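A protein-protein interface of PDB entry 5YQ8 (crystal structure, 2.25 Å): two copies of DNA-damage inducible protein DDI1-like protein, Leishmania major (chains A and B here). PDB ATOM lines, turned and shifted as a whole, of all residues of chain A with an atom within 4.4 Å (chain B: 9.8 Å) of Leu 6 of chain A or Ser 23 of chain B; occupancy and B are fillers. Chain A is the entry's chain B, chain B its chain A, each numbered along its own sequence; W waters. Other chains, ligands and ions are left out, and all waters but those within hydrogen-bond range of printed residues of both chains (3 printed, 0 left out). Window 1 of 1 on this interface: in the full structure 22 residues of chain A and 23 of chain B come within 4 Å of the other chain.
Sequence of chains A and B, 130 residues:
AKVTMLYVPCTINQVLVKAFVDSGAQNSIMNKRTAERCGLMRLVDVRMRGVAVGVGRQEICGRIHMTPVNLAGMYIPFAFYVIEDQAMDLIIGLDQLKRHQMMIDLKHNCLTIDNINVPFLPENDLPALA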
ATOM      1  N   THR A   4     -23.721  36.129 -31.112  1.00  0.00           N
ATOM      2  CA  THR A   4     -24.300  36.686 -29.942  1.00  0.00           C
ATOM      3  C   THR A   4     -24.490  35.601 -28.816  1.00  0.00           C
ATOM      4  O   THR A   4     -25.048  34.508 -29.055  1.00  0.00           O
ATOM      5  CB  THR A   4     -25.637  37.301 -30.301  1.00  0.00           C
ATOM      6  OG1 THR A   4     -25.518  38.104 -31.487  1.00  0.00           O
ATOM      7  CG2 THR A   4     -26.106  38.173 -29.145  1.00  0.00           C
ATOM      8  N   MET A   5     -24.048  35.942 -27.605  1.00  0.00           N
ATOM      9  CA  MET A   5     -24.245  35.085 -26.473  1.00  0.00           C
ATOM     10  C   MET A   5     -25.699  35.078 -26.079  1.00  0.00           C
ATOM     11  O   MET A   5     -26.471  35.850 -26.572  1.00  0.00           O
ATOM     12  CB  MET A   5     -23.381  35.477 -25.281  1.00  0.00           C
ATOM     13  CG  MET A   5     -21.866  35.507 -25.538  1.00  0.00           C
ATOM     14  SD  MET A   5     -21.065  33.956 -26.031  1.00  0.00           S
ATOM     15  CE  MET A   5     -21.178  34.193 -27.773  1.00  0.00           C
ATOM     16  N   LEU A   6     -26.051  34.130 -25.246  1.00  0.00           N
ATOM     17  CA  LEU A   6     -27.416  33.910 -24.836  1.00  0.00           C
ATOM     18  C   LEU A   6     -27.884  34.892 -23.775  1.00  0.00           C
ATOM     19  O   LEU A   6     -27.416  34.827 -22.666  1.00  0.00           O
ATOM     20  CB  LEU A   6     -27.482  32.482 -24.363  1.00  0.00           C
ATOM     21  CG  LEU A   6     -27.102  31.408 -25.406  1.00  0.00           C
ATOM     22  CD1 LEU A   6     -27.418  30.053 -24.885  1.00  0.00           C
ATOM     23  CD2 LEU A   6     -27.892  31.544 -26.676  1.00  0.00           C
ATOM     24  N   TYR A   7     -28.762  35.828 -24.124  1.00  0.00           N
ATOM     25  CA  TYR A   7     -29.396  36.719 -23.166  1.00  0.00           C
ATOM     26  C   TYR A   7     -30.918  36.675 -23.301  1.00  0.00           C
ATOM     27  O   TYR A   7     -31.472  36.586 -24.396  1.00  0.00           O
ATOM     28  CB  TYR A   7     -28.969  38.137 -23.391  1.00  0.00           C
ATOM     29  CG  TYR A   7     -27.570  38.466 -22.965  1.00  0.00           C
ATOM     30  CD1 TYR A   7     -26.486  38.268 -23.830  1.00  0.00           C
ATOM     31  CD2 TYR A   7     -27.331  39.045 -21.729  1.00  0.00           C
ATOM     32  CE1 TYR A   7     -25.215  38.573 -23.427  1.00  0.00           C
ATOM     33  CE2 TYR A   7     -26.072  39.357 -21.318  1.00  0.00           C
ATOM     34  CZ  TYR A   7     -25.036  39.148 -22.178  1.00  0.00           C
ATOM     35  OH  TYR A   7     -23.797  39.543 -21.740  1.00  0.00           O
ATOM     36  N   ALA A  19     -30.842  38.680 -18.508  1.00  0.00           N
ATOM     37  CA  ALA A  19     -30.083  37.578 -17.917  1.00  0.00           C
ATOM     38  C   ALA A  19     -29.257  36.802 -18.959  1.00  0.00           C
ATOM     39  O   ALA A  19     -29.710  36.469 -20.042  1.00  0.00           O
ATOM     40  CB  ALA A  19     -31.049  36.672 -17.177  1.00  0.00           C
ATOM     41  N   PHE A  20     -28.016  36.533 -18.628  1.00  0.00           N
ATOM     42  CA  PHE A  20     -27.121  35.764 -19.460  1.00  0.00           C
ATOM     43  C   PHE A  20     -27.221  34.298 -19.106  1.00  0.00           C
ATOM     44  O   PHE A  20     -26.953  33.904 -17.986  1.00  0.00           O
ATOM     45  CB  PHE A  20     -25.714  36.255 -19.170  1.00  0.00           C
ATOM     46  CG  PHE A  20     -24.623  35.549 -19.914  1.00  0.00           C
ATOM     47  CD1 PHE A  20     -24.477  35.728 -21.240  1.00  0.00           C
ATOM     48  CD2 PHE A  20     -23.700  34.741 -19.247  1.00  0.00           C
ATOM     49  CE1 PHE A  20     -23.434  35.124 -21.916  1.00  0.00           C
ATOM     50  CE2 PHE A  20     -22.630  34.150 -19.921  1.00  0.00           C
ATOM     51  CZ  PHE A  20     -22.518  34.333 -21.262  1.00  0.00           C
ATOM     52  N   VAL A  21     -27.604  33.494 -20.069  1.00  0.00           N
ATOM     53  CA  VAL A  21     -27.854  32.085 -19.883  1.00  0.00           C
ATOM     54  C   VAL A  21     -26.580  31.319 -20.234  1.00  0.00           C
ATOM     55  O   VAL A  21     -26.114  31.339 -21.372  1.00  0.00           O
ATOM     56  CB  VAL A  21     -29.039  31.620 -20.775  1.00  0.00           C
ATOM     57  CG1 VAL A  21     -29.468  30.158 -20.451  1.00  0.00           C
ATOM     58  CG2 VAL A  21     -30.183  32.620 -20.575  1.00  0.00           C
ATOM     59  N   ASP A  22     -26.021  30.657 -19.228  1.00  0.00           N
ATOM     60  CA  ASP A  22     -24.777  29.960 -19.305  1.00  0.00           C
ATOM     61  C   ASP A  22     -24.920  28.607 -18.650  1.00  0.00           C
ATOM     62  O   ASP A  22     -24.920  28.511 -17.417  1.00  0.00           O
ATOM     63  CB  ASP A  22     -23.642  30.780 -18.632  1.00  0.00           C
ATOM     64  CG  ASP A  22     -22.371  29.996 -18.488  1.00  0.00           C
ATOM     65  OD1 ASP A  22     -22.136  29.090 -19.286  1.00  0.00           O
ATOM     66  OD2 ASP A  22     -21.573  30.267 -17.598  1.00  0.00           O
ATOM     67  N   SER A  23     -24.966  27.565 -19.477  1.00  0.00           N
ATOM     68  CA  SER A  23     -25.032  26.188 -19.047  1.00  0.00           C
ATOM     69  C   SER A  23     -23.722  25.640 -18.512  1.00  0.00           C
ATOM     70  O   SER A  23     -23.680  24.475 -18.065  1.00  0.00           O
ATOM     71  CB  SER A  23     -25.482  25.290 -20.200  1.00  0.00           C
ATOM     72  OG  SER A  23     -24.371  24.991 -21.008  1.00  0.00           O
ATOM     73  N   GLY A  24     -22.652  26.437 -18.561  1.00  0.00           N
ATOM     74  CA  GLY A  24     -21.374  26.030 -18.027  1.00  0.00           C
ATOM     75  C   GLY A  24     -21.113  26.618 -16.676  1.00  0.00           C
ATOM     76  O   GLY A  24     -20.007  26.514 -16.197  1.00  0.00           O
ATOM     77  N   ILE A 104     -32.647  25.097 -23.702  1.00  0.00           N
ATOM     78  CA  ILE A 104     -31.936  26.085 -24.459  1.00  0.00           C
ATOM     79  C   ILE A 104     -32.138  25.668 -25.880  1.00  0.00           C
ATOM     80  O   ILE A 104     -31.522  24.722 -26.347  1.00  0.00           O
ATOM     81  CB  ILE A 104     -30.451  26.181 -24.094  1.00  0.00           C
ATOM     82  CG1 ILE A 104     -30.225  26.537 -22.612  1.00  0.00           C
ATOM     83  CG2 ILE A 104     -29.793  27.243 -24.923  1.00  0.00           C
ATOM     84  CD1 ILE A 104     -28.890  26.103 -22.030  1.00  0.00           C
ATOM     85  N   LEU A 106     -31.688  26.510 -29.735  1.00  0.00           N
ATOM     86  CA  LEU A 106     -31.007  27.309 -30.750  1.00  0.00           C
ATOM     87  C   LEU A 106     -31.396  26.991 -32.205  1.00  0.00           C
ATOM     88  O   LEU A 106     -30.954  27.728 -33.123  1.00  0.00           O
ATOM     89  CB  LEU A 106     -29.508  27.150 -30.645  1.00  0.00           C
ATOM     90  CG  LEU A 106     -28.961  27.290 -29.230  1.00  0.00           C
ATOM     91  CD1 LEU A 106     -27.581  26.732 -29.265  1.00  0.00           C
ATOM     92  CD2 LEU A 106     -28.901  28.705 -28.686  1.00  0.00           C
ATOM     93  N   PHE A 120     -34.344  34.754 -27.760  1.00  0.00           N
ATOM     94  CA  PHE A 120     -33.057  35.335 -27.340  1.00  0.00           C
ATOM     95  C   PHE A 120     -32.885  36.695 -27.982  1.00  0.00           C
ATOM     96  O   PHE A 120     -33.452  36.989 -29.029  1.00  0.00           O
ATOM     97  CB  PHE A 120     -31.888  34.422 -27.709  1.00  0.00           C
ATOM     98  CG  PHE A 120     -31.916  33.087 -27.042  1.00  0.00           C
ATOM     99  CD1 PHE A 120     -32.271  32.970 -25.720  1.00  0.00           C
ATOM    100  CD2 PHE A 120     -31.533  31.944 -27.731  1.00  0.00           C
ATOM    101  CE1 PHE A 120     -32.279  31.737 -25.129  1.00  0.00           C
ATOM    102  CE2 PHE A 120     -31.543  30.736 -27.140  1.00  0.00           C
ATOM    103  CZ  PHE A 120     -31.917  30.638 -25.842  1.00  0.00           C
ATOM    104  N   LEU B   6     -22.662  19.438 -17.745  1.00  0.00           N
ATOM    105  CA  LEU B   6     -23.179  18.738 -18.953  1.00  0.00           C
ATOM    106  C   LEU B   6     -22.026  18.264 -19.830  1.00  0.00           C
ATOM    107  O   LEU B   6     -21.278  19.077 -20.346  1.00  0.00           O
ATOM    108  CB  LEU B   6     -24.082  19.641 -19.819  1.00  0.00           C
ATOM    109  CG  LEU B   6     -25.263  20.268 -19.104  1.00  0.00           C
ATOM    110  CD1 LEU B   6     -26.184  21.027 -20.091  1.00  0.00           C
ATOM    111  CD2 LEU B   6     -26.054  19.171 -18.333  1.00  0.00           C
ATOM    112  N   PHE B  20     -17.665  18.814 -23.170  1.00  0.00           N
ATOM    113  CA  PHE B  20     -18.412  19.756 -22.305  1.00  0.00           C
ATOM    114  C   PHE B  20     -19.299  20.720 -23.082  1.00  0.00           C
ATOM    115  O   PHE B  20     -18.821  21.314 -24.031  1.00  0.00           O
ATOM    116  CB  PHE B  20     -17.415  20.560 -21.530  1.00  0.00           C
ATOM    117  CG  PHE B  20     -18.010  21.462 -20.473  1.00  0.00           C
ATOM    118  CD1 PHE B  20     -18.598  20.925 -19.348  1.00  0.00           C
ATOM    119  CD2 PHE B  20     -17.904  22.866 -20.575  1.00  0.00           C
ATOM    120  CE1 PHE B  20     -19.056  21.754 -18.336  1.00  0.00           C
ATOM    121  CE2 PHE B  20     -18.412  23.680 -19.593  1.00  0.00           C
ATOM    122  CZ  PHE B  20     -19.011  23.127 -18.477  1.00  0.00           C
ATOM    123  N   VAL B  21     -20.557  20.825 -22.680  1.00  0.00           N
ATOM    124  CA  VAL B  21     -21.559  21.603 -23.414  1.00  0.00           C
ATOM    125  C   VAL B  21     -21.808  22.916 -22.670  1.00  0.00           C
ATOM    126  O   VAL B  21     -22.536  22.916 -21.657  1.00  0.00           O
ATOM    127  CB  VAL B  21     -22.878  20.848 -23.551  1.00  0.00           C
ATOM    128  CG1 VAL B  21     -23.950  21.739 -24.186  1.00  0.00           C
ATOM    129  CG2 VAL B  21     -22.697  19.522 -24.328  1.00  0.00           C
ATOM    130  N   ASP B  22     -21.224  23.999 -23.174  1.00  0.00           N
ATOM    131  CA  ASP B  22     -21.074  25.295 -22.446  1.00  0.00           C
ATOM    132  C   ASP B  22     -21.720  26.402 -23.207  1.00  0.00           C
ATOM    133  O   ASP B  22     -21.144  26.897 -24.139  1.00  0.00           O
ATOM    134  CB  ASP B  22     -19.582  25.603 -22.289  1.00  0.00           C
ATOM    135  CG  ASP B  22     -19.277  26.744 -21.351  1.00  0.00           C
ATOM    136  OD1 ASP B  22     -20.204  27.457 -20.922  1.00  0.00           O
ATOM    137  OD2 ASP B  22     -18.051  26.932 -21.084  1.00  0.00           O
ATOM    138  N   SER B  23     -22.927  26.786 -22.848  1.00  0.00           N
ATOM    139  CA  SER B  23     -23.676  27.799 -23.599  1.00  0.00           C
ATOM    140  C   SER B  23     -23.159  29.185 -23.370  1.00  0.00           C
ATOM    141  O   SER B  23     -23.402  30.063 -24.170  1.00  0.00           O
ATOM    142  CB  SER B  23     -25.187  27.707 -23.277  1.00  0.00           C
ATOM    143  OG  SER B  23     -25.558  28.407 -22.080  1.00  0.00           O
ATOM    144  N   GLY B  24     -22.425  29.385 -22.297  1.00  0.00           N
ATOM    145  CA  GLY B  24     -21.651  30.600 -22.095  1.00  0.00           C
ATOM    146  C   GLY B  24     -20.275  30.720 -22.691  1.00  0.00           C
ATOM    147  O   GLY B  24     -19.608  31.704 -22.448  1.00  0.00           O
ATOM    148  N   ALA B  25     -19.805  29.725 -23.427  1.00  0.00           N
ATOM    149  CA  ALA B  25     -18.476  29.796 -24.105  1.00  0.00           C
ATOM    150  C   ALA B  25     -18.724  30.188 -25.545  1.00  0.00           C
ATOM    151  O   ALA B  25     -19.446  29.507 -26.276  1.00  0.00           O
ATOM    152  CB  ALA B  25     -17.762  28.460 -24.060  1.00  0.00           C
ATOM    153  N   GLN B  26     -18.146  31.297 -25.949  1.00  0.00           N
ATOM    154  CA  GLN B  26     -18.271  31.689 -27.328  1.00  0.00           C
ATOM    155  C   GLN B  26     -17.505  30.741 -28.289  1.00  0.00           C
ATOM    156  O   GLN B  26     -17.970  30.554 -29.382  1.00  0.00           O
ATOM    157  CB  GLN B  26     -17.837  33.150 -27.525  1.00  0.00           C
ATOM    158  CG  GLN B  26     -18.082  33.635 -28.941  1.00  0.00           C
ATOM    159  CD  GLN B  26     -18.163  35.131 -29.043  1.00  0.00           C
ATOM    160  OE1 GLN B  26     -19.264  35.727 -29.209  1.00  0.00           O
ATOM    161  NE2 GLN B  26     -16.992  35.768 -28.971  1.00  0.00           N
ATOM    162  N   ASN B  27     -16.374  30.160 -27.900  1.00  0.00           N
ATOM    163  CA  ASN B  27     -15.558  29.322 -28.833  1.00  0.00           C
ATOM    164  C   ASN B  27     -15.526  27.857 -28.380  1.00  0.00           C
ATOM    165  O   ASN B  27     -15.505  27.572 -27.183  1.00  0.00           O
ATOM    166  CB  ASN B  27     -14.135  29.885 -28.916  1.00  0.00           C
ATOM    167  CG  ASN B  27     -14.114  31.348 -29.375  1.00  0.00           C
ATOM    168  OD1 ASN B  27     -14.189  31.628 -30.610  1.00  0.00           O
ATOM    169  ND2 ASN B  27     -14.100  32.291 -28.393  1.00  0.00           N
ATOM    170  N   SER B  28     -15.555  26.945 -29.351  1.00  0.00           N
ATOM    171  CA  SER B  28     -15.175  25.544 -29.123  1.00  0.00           C
ATOM    172  C   SER B  28     -13.662  25.390 -29.126  1.00  0.00           C
ATOM    173  O   SER B  28     -12.975  26.013 -29.939  1.00  0.00           O
ATOM    174  CB  SER B  28     -15.796  24.614 -30.160  1.00  0.00           C
ATOM    175  OG  SER B  28     -17.199  24.503 -29.949  1.00  0.00           O
ATOM    176  N   MET B  88     -10.099  20.289 -19.792  1.00  0.00           N
ATOM    177  CA  MET B  88     -11.219  19.601 -20.433  1.00  0.00           C
ATOM    178  C   MET B  88     -10.878  19.283 -21.862  1.00  0.00           C
ATOM    179  O   MET B  88     -10.450  20.165 -22.636  1.00  0.00           O
ATOM    180  CB  MET B  88     -12.513  20.435 -20.376  1.00  0.00           C
ATOM    181  CG  MET B  88     -12.877  20.740 -18.961  1.00  0.00           C
ATOM    182  SD  MET B  88     -14.564  21.307 -18.854  1.00  0.00           S
ATOM    183  CE  MET B  88     -14.546  22.924 -19.620  1.00  0.00           C
ATOM    184  N   ILE B  91     -14.614  21.217 -25.517  1.00  0.00           N
ATOM    185  CA  ILE B  91     -15.679  22.086 -25.174  1.00  0.00           C
ATOM    186  C   ILE B  91     -16.517  22.382 -26.441  1.00  0.00           C
ATOM    187  O   ILE B  91     -15.974  22.903 -27.467  1.00  0.00           O
ATOM    188  CB  ILE B  91     -15.136  23.380 -24.568  1.00  0.00           C
ATOM    189  CG1 ILE B  91     -14.172  23.009 -23.440  1.00  0.00           C
ATOM    190  CG2 ILE B  91     -16.281  24.174 -24.023  1.00  0.00           C
ATOM    191  CD1 ILE B  91     -13.479  24.147 -22.763  1.00  0.00           C
ATOM    192  N   ILE B  92     -17.806  22.007 -26.371  1.00  0.00           N
ATOM    193  CA  ILE B  92     -18.796  22.409 -27.321  1.00  0.00           C
ATOM    194  C   ILE B  92     -19.287  23.815 -26.932  1.00  0.00           C
ATOM    195  O   ILE B  92     -20.013  23.977 -25.968  1.00  0.00           O
ATOM    196  CB  ILE B  92     -19.929  21.421 -27.340  1.00  0.00           C
ATOM    197  CG1 ILE B  92     -19.410  20.078 -27.812  1.00  0.00           C
ATOM    198  CG2 ILE B  92     -21.027  21.870 -28.317  1.00  0.00           C
ATOM    199  CD1 ILE B  92     -20.495  19.042 -27.918  1.00  0.00           C
ATOM    200  N   GLY B  93     -18.865  24.841 -27.656  1.00  0.00           N
ATOM    201  CA  GLY B  93     -19.327  26.206 -27.354  1.00  0.00           C
ATOM    202  C   GLY B  93     -20.595  26.593 -28.091  1.00  0.00           C
ATOM    203  O   GLY B  93     -21.191  25.837 -28.888  1.00  0.00           O
ATOM    204  N   LEU B  94     -20.978  27.828 -27.856  1.00  0.00           N
ATOM    205  CA  LEU B  94     -22.112  28.455 -28.517  1.00  0.00           C
ATOM    206  C   LEU B  94     -21.961  28.590 -30.048  1.00  0.00           C
ATOM    207  O   LEU B  94     -22.925  28.581 -30.737  1.00  0.00           O
ATOM    208  CB  LEU B  94     -22.338  29.821 -27.852  1.00  0.00           C
ATOM    209  CG  LEU B  94     -23.745  30.421 -27.931  1.00  0.00           C
ATOM    210  CD1 LEU B  94     -24.752  29.410 -27.426  1.00  0.00           C
ATOM    211  CD2 LEU B  94     -23.796  31.725 -27.176  1.00  0.00           C
ATOM    212  N   ASP B  95     -20.774  28.693 -30.598  1.00  0.00           N
ATOM    213  CA  ASP B  95     -20.623  28.587 -32.043  1.00  0.00           C
ATOM    214  C   ASP B  95     -21.215  27.300 -32.659  1.00  0.00           C
ATOM    215  O   ASP B  95     -21.994  27.342 -33.632  1.00  0.00           O
ATOM    216  CB  ASP B  95     -19.134  28.690 -32.423  1.00  0.00           C
ATOM    217  CG  ASP B  95     -18.178  28.078 -31.356  1.00  0.00           C
ATOM    218  OD1 ASP B  95     -18.619  27.840 -30.167  1.00  0.00           O
ATOM    219  OD2 ASP B  95     -16.978  27.918 -31.697  1.00  0.00           O
ATOM    220  N   GLN B  96     -20.807  26.144 -32.151  1.00  0.00           N
ATOM    221  CA  GLN B  96     -21.251  24.852 -32.702  1.00  0.00           C
ATOM    222  C   GLN B  96     -22.664  24.485 -32.240  1.00  0.00           C
ATOM    223  O   GLN B  96     -23.424  23.925 -32.965  1.00  0.00           O
ATOM    224  CB  GLN B  96     -20.254  23.730 -32.344  1.00  0.00           C
ATOM    225  CG  GLN B  96     -18.847  23.916 -32.923  1.00  0.00           C
ATOM    226  CD  GLN B  96     -18.805  23.775 -34.401  1.00  0.00           C
ATOM    227  OE1 GLN B  96     -19.540  22.962 -34.953  1.00  0.00           O
ATOM    228  NE2 GLN B  96     -17.946  24.534 -35.053  1.00  0.00           N
ATOM    229  N   LEU B  97     -23.041  24.857 -31.022  1.00  0.00           N
ATOM    230  CA  LEU B  97     -24.443  24.742 -30.587  1.00  0.00           C
ATOM    231  C   LEU B  97     -25.386  25.481 -31.513  1.00  0.00           C
ATOM    232  O   LEU B  97     -26.434  24.967 -31.858  1.00  0.00           O
ATOM    233  CB  LEU B  97     -24.612  25.256 -29.172  1.00  0.00           C
ATOM    234  CG  LEU B  97     -24.159  24.337 -28.022  1.00  0.00           C
ATOM    235  CD1 LEU B  97     -24.235  25.019 -26.696  1.00  0.00           C
ATOM    236  CD2 LEU B  97     -25.000  23.071 -28.019  1.00  0.00           C
ATOM    237  N   LYS B  98     -24.996  26.675 -31.921  1.00  0.00           N
ATOM    238  CA  LYS B  98     -25.696  27.441 -32.935  1.00  0.00           C
ATOM    239  C   LYS B  98     -25.481  26.994 -34.365  1.00  0.00           C
ATOM    240  O   LYS B  98     -26.406  26.872 -35.116  1.00  0.00           O
ATOM    241  CB  LYS B  98     -25.355  28.933 -32.809  1.00  0.00           C
ATOM    242  CG  LYS B  98     -25.846  29.576 -31.532  1.00  0.00           C
ATOM    243  CD  LYS B  98     -26.053  31.052 -31.827  1.00  0.00           C
ATOM    244  CE  LYS B  98     -27.132  31.659 -31.000  1.00  0.00           C
ATOM    245  NZ  LYS B  98     -26.933  33.096 -31.102  1.00  0.00           N
ATOM    246  N   MET B 102     -28.493  23.013 -32.273  1.00  0.00           N
ATOM    247  CA  MET B 102     -28.676  22.045 -31.217  1.00  0.00           C
ATOM    248  C   MET B 102     -29.690  22.534 -30.196  1.00  0.00           C
ATOM    249  O   MET B 102     -30.063  23.693 -30.156  1.00  0.00           O
ATOM    250  CB  MET B 102     -27.313  21.684 -30.543  1.00  0.00           C
ATOM    251  CG  MET B 102     -26.353  21.012 -31.493  1.00  0.00           C
ATOM    252  SD  MET B 102     -24.796  20.637 -30.663  1.00  0.00           S
ATOM    253  CE  MET B 102     -23.650  20.389 -32.029  1.00  0.00           C
ATOM    254  N   MET B 103     -30.113  21.595 -29.356  1.00  0.00           N
ATOM    255  CA  MET B 103     -31.063  21.833 -28.321  1.00  0.00           C
ATOM    256  C   MET B 103     -30.500  21.196 -27.063  1.00  0.00           C
ATOM    257  O   MET B 103     -30.176  19.996 -27.031  1.00  0.00           O
ATOM    258  CB  MET B 103     -32.434  21.272 -28.703  1.00  0.00           C
ATOM    259  CG  MET B 103     -33.101  21.887 -29.975  1.00  0.00           C
ATOM    260  SD  MET B 103     -34.423  20.925 -30.802  1.00  0.00           S
ATOM    261  CE  MET B 103     -34.585  21.722 -32.394  1.00  0.00           C
ATOM    262  N   ILE B 104     -30.428  22.002 -25.997  1.00  0.00           N
ATOM    263  CA  ILE B 104     -29.903  21.574 -24.713  1.00  0.00           C
ATOM    264  C   ILE B 104     -31.119  21.415 -23.837  1.00  0.00           C
ATOM    265  O   ILE B 104     -31.623  22.394 -23.228  1.00  0.00           O
ATOM    266  CB  ILE B 104     -28.923  22.575 -24.121  1.00  0.00           C
ATOM    267  CG1 ILE B 104     -27.766  22.848 -25.096  1.00  0.00           C
ATOM    268  CG2 ILE B 104     -28.308  22.092 -22.807  1.00  0.00           C
ATOM    269  CD1 ILE B 104     -27.063  24.182 -24.797  1.00  0.00           C
ATOM    270  N   LEU B 106     -32.829  20.146 -20.786  1.00  0.00           N
ATOM    271  CA  LEU B 106     -32.650  19.790 -19.380  1.00  0.00           C
ATOM    272  C   LEU B 106     -33.933  19.372 -18.706  1.00  0.00           C
ATOM    273  O   LEU B 106     -34.010  19.333 -17.469  1.00  0.00           O
ATOM    274  CB  LEU B 106     -32.072  20.944 -18.573  1.00  0.00           C
ATOM    275  CG  LEU B 106     -30.743  21.416 -19.083  1.00  0.00           C
ATOM    276  CD1 LEU B 106     -30.563  22.907 -18.775  1.00  0.00           C
ATOM    277  CD2 LEU B 106     -29.649  20.544 -18.534  1.00  0.00           C
ATOM    278  N   LEU B 111     -29.074  16.011 -25.376  1.00  0.00           N
ATOM    279  CA  LEU B 111     -28.635  16.962 -26.372  1.00  0.00           C
ATOM    280  C   LEU B 111     -29.211  16.557 -27.674  1.00  0.00           C
ATOM    281  O   LEU B 111     -28.878  15.470 -28.177  1.00  0.00           O
ATOM    282  CB  LEU B 111     -27.143  16.983 -26.494  1.00  0.00           C
ATOM    283  CG  LEU B 111     -26.533  18.022 -27.451  1.00  0.00           C
ATOM    284  CD1 LEU B 111     -26.749  19.453 -26.966  1.00  0.00           C
ATOM    285  CD2 LEU B 111     -25.029  17.744 -27.618  1.00  0.00           C
ATOM    286  N   PHE B 120     -26.965  13.288 -21.525  1.00  0.00           N
ATOM    287  CA  PHE B 120     -25.832  13.793 -20.785  1.00  0.00           C
ATOM    288  C   PHE B 120     -25.365  12.688 -19.911  1.00  0.00           C
ATOM    289  O   PHE B 120     -26.195  11.902 -19.321  1.00  0.00           O
ATOM    290  CB  PHE B 120     -26.198  15.030 -19.956  1.00  0.00           C
ATOM    291  CG  PHE B 120     -26.591  16.211 -20.820  1.00  0.00           C
ATOM    292  CD1 PHE B 120     -25.714  16.718 -21.782  1.00  0.00           C
ATOM    293  CD2 PHE B 120     -27.866  16.776 -20.724  1.00  0.00           C
ATOM    294  CE1 PHE B 120     -26.116  17.764 -22.638  1.00  0.00           C
ATOM    295  CE2 PHE B 120     -28.247  17.825 -21.572  1.00  0.00           C
ATOM    296  CZ  PHE B 120     -27.368  18.318 -22.530  1.00  0.00           C
HETATM  297  O   HOH W   1     -29.261  24.544 -27.635  1.00  0.00           O
HETATM  298  O   HOH W   2     -24.197  32.365 -23.626  1.00  0.00           O
HETATM  299  O   HOH W   3     -20.222  31.609 -19.454  1.00  0.00           O
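Of the 25 printed residues of chain B, 12 touch a printed residue of chain A.
Printed residues of chain B that touch a printed residue of chain A: Phe 20, Val 21, Asp 22, Ser 23, Gly 24, Gln 26, Leu 94, Leu 97, Lys 98, Met 102, Met 103 and Ile 104.
CA of Met 5 of chain A touches CD2 of Leu 94 of chain B, 3.5 Å away.
Leu 6 of chain A touches Ser 23 of chain B (CD1 to CB, 3.6 Å).
Leu 6 of chain A touches Leu 94 of chain B.
Phe 20 of chain A touches Gly 24 of chain B.
CA of Gly 24 of chain A touches CZ of Phe 20 of chain B, 3.8 Å away.
CB of Leu 97 of chain B touches CD1 of Leu 106 of chain A, 3.3 Å away.
Water W2 lies within hydrogen-bond range of the backbone carbonyl oxygen (O) of Ser 23 of chain B (2.5 Å), the backbone NH (N) of Leu 6 of chain A (3.0 Å) and the backbone carbonyl oxygen (O) of Val 21 of chain A (3.1 Å).
Leu 6 of chain A touches Ser 23 of chain B, but with the chains exchanged Ser 23 of chain A does not touch Leu 6 of chain B (4.3 Å).
Val 21 of chain A touches Ser 23 of chain B, and with the chains exchanged Ser 23 of chain A touches Val 21 of chain B.
Asp 22 of chain A touches its own counterpart, Asp 22 of chain B.
Of chain B, only Gln 26 (2.8 Å) and Leu 94 (3.5 Å) come within 4 Å of Met 5 of chain A.
Of chain B, only Ser 23 and Leu 94 come within 4 Å of Leu 6 of chain A.
Phe 20 of chain A touches just one residue of chain B: Gly 24 (3.9 Å).
Printed residues of chain B within 4 Å of Val 21 of chain A: Ser 23.
Printed residues of chain B within 4 Å of Ile 104 of chain A: Met 103 (3.5 Å) and Ile 104 (2.9 Å).
Ser 23 of chain B touches just these residues of chain A: Leu 6 (3.6 Å), Val 21 (3.1 Å), Asp 22 (3.3 Å) and Ser 23 (2.8 Å).
Of the printed residues of chain A, Leu 94 of chain B touches Thr 4, Met 5 and Leu 6.
Printed residues of chain A within 4 Å of Met 103 of chain B: Ile 104.
The nearest residue of chain B that does not touch Leu 6 of chain A is Lys 98 of chain B (4.4 Å).
The nearest residue of chain A that does not touch Ser 23 of chain B is Ile 104 of chain A (4.1 Å).
The nearest printed residue of chain B that does not touch Thr 4 of chain A is Gln 26 of chain B (4.9 Å).
The backbone carbonyl oxygen of Met 102 of chain B sits at hydrogen-bond distance from the backbone NH of Leu 106 of chain A, 3.3 Å away.
The side-chain amino group (NZ) of Lys 98 of chain B is in hydrogen-bond range of the backbone carbonyl oxygen (O) of Thr 4 of chain A (3.1 Å).
The side-chain carboxylate (OD1) of Asp 22 of chain A lies close to the side-chain carboxylate (OD1) of Asp 22 of chain B, 3.0 Å away.
N of Gly 24 of chain B sits at hydrogen-bond distance from OD1 of Asp 22 of chain A (3.0 Å).
The side-chain hydroxyl (OG) of Ser 23 of chain B is in hydrogen-bond range of the backbone NH (N) of Ser 23 of chain A, at 2.8 Å.
OG of Ser 23 of chain A sits at hydrogen-bond distance from O of Val 21 of chain B (2.8 Å).
The side-chain hydroxyl of Ser 23 of chain B lies within hydrogen-bond range of the backbone carbonyl oxygen of Val 21 of chain A (3.1 Å).
O of Ile 104 of chain B lies within hydrogen-bond range of N of Ile 104 of chain A.
The backbone NH (N) of Gly 24 of chain A is in hydrogen-bond range of the side-chain carboxylate (OD1) of Asp 22 of chain A, at 2.8 Å.
The side-chain carboxylate (OD1) of Asp 22 of chain B lies close to the backbone NH (N) of Gly 24 of chain B (3.2 Å).
N of Leu 94 of chain B sits at hydrogen-bond distance from O of Ala 25 of chain B.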
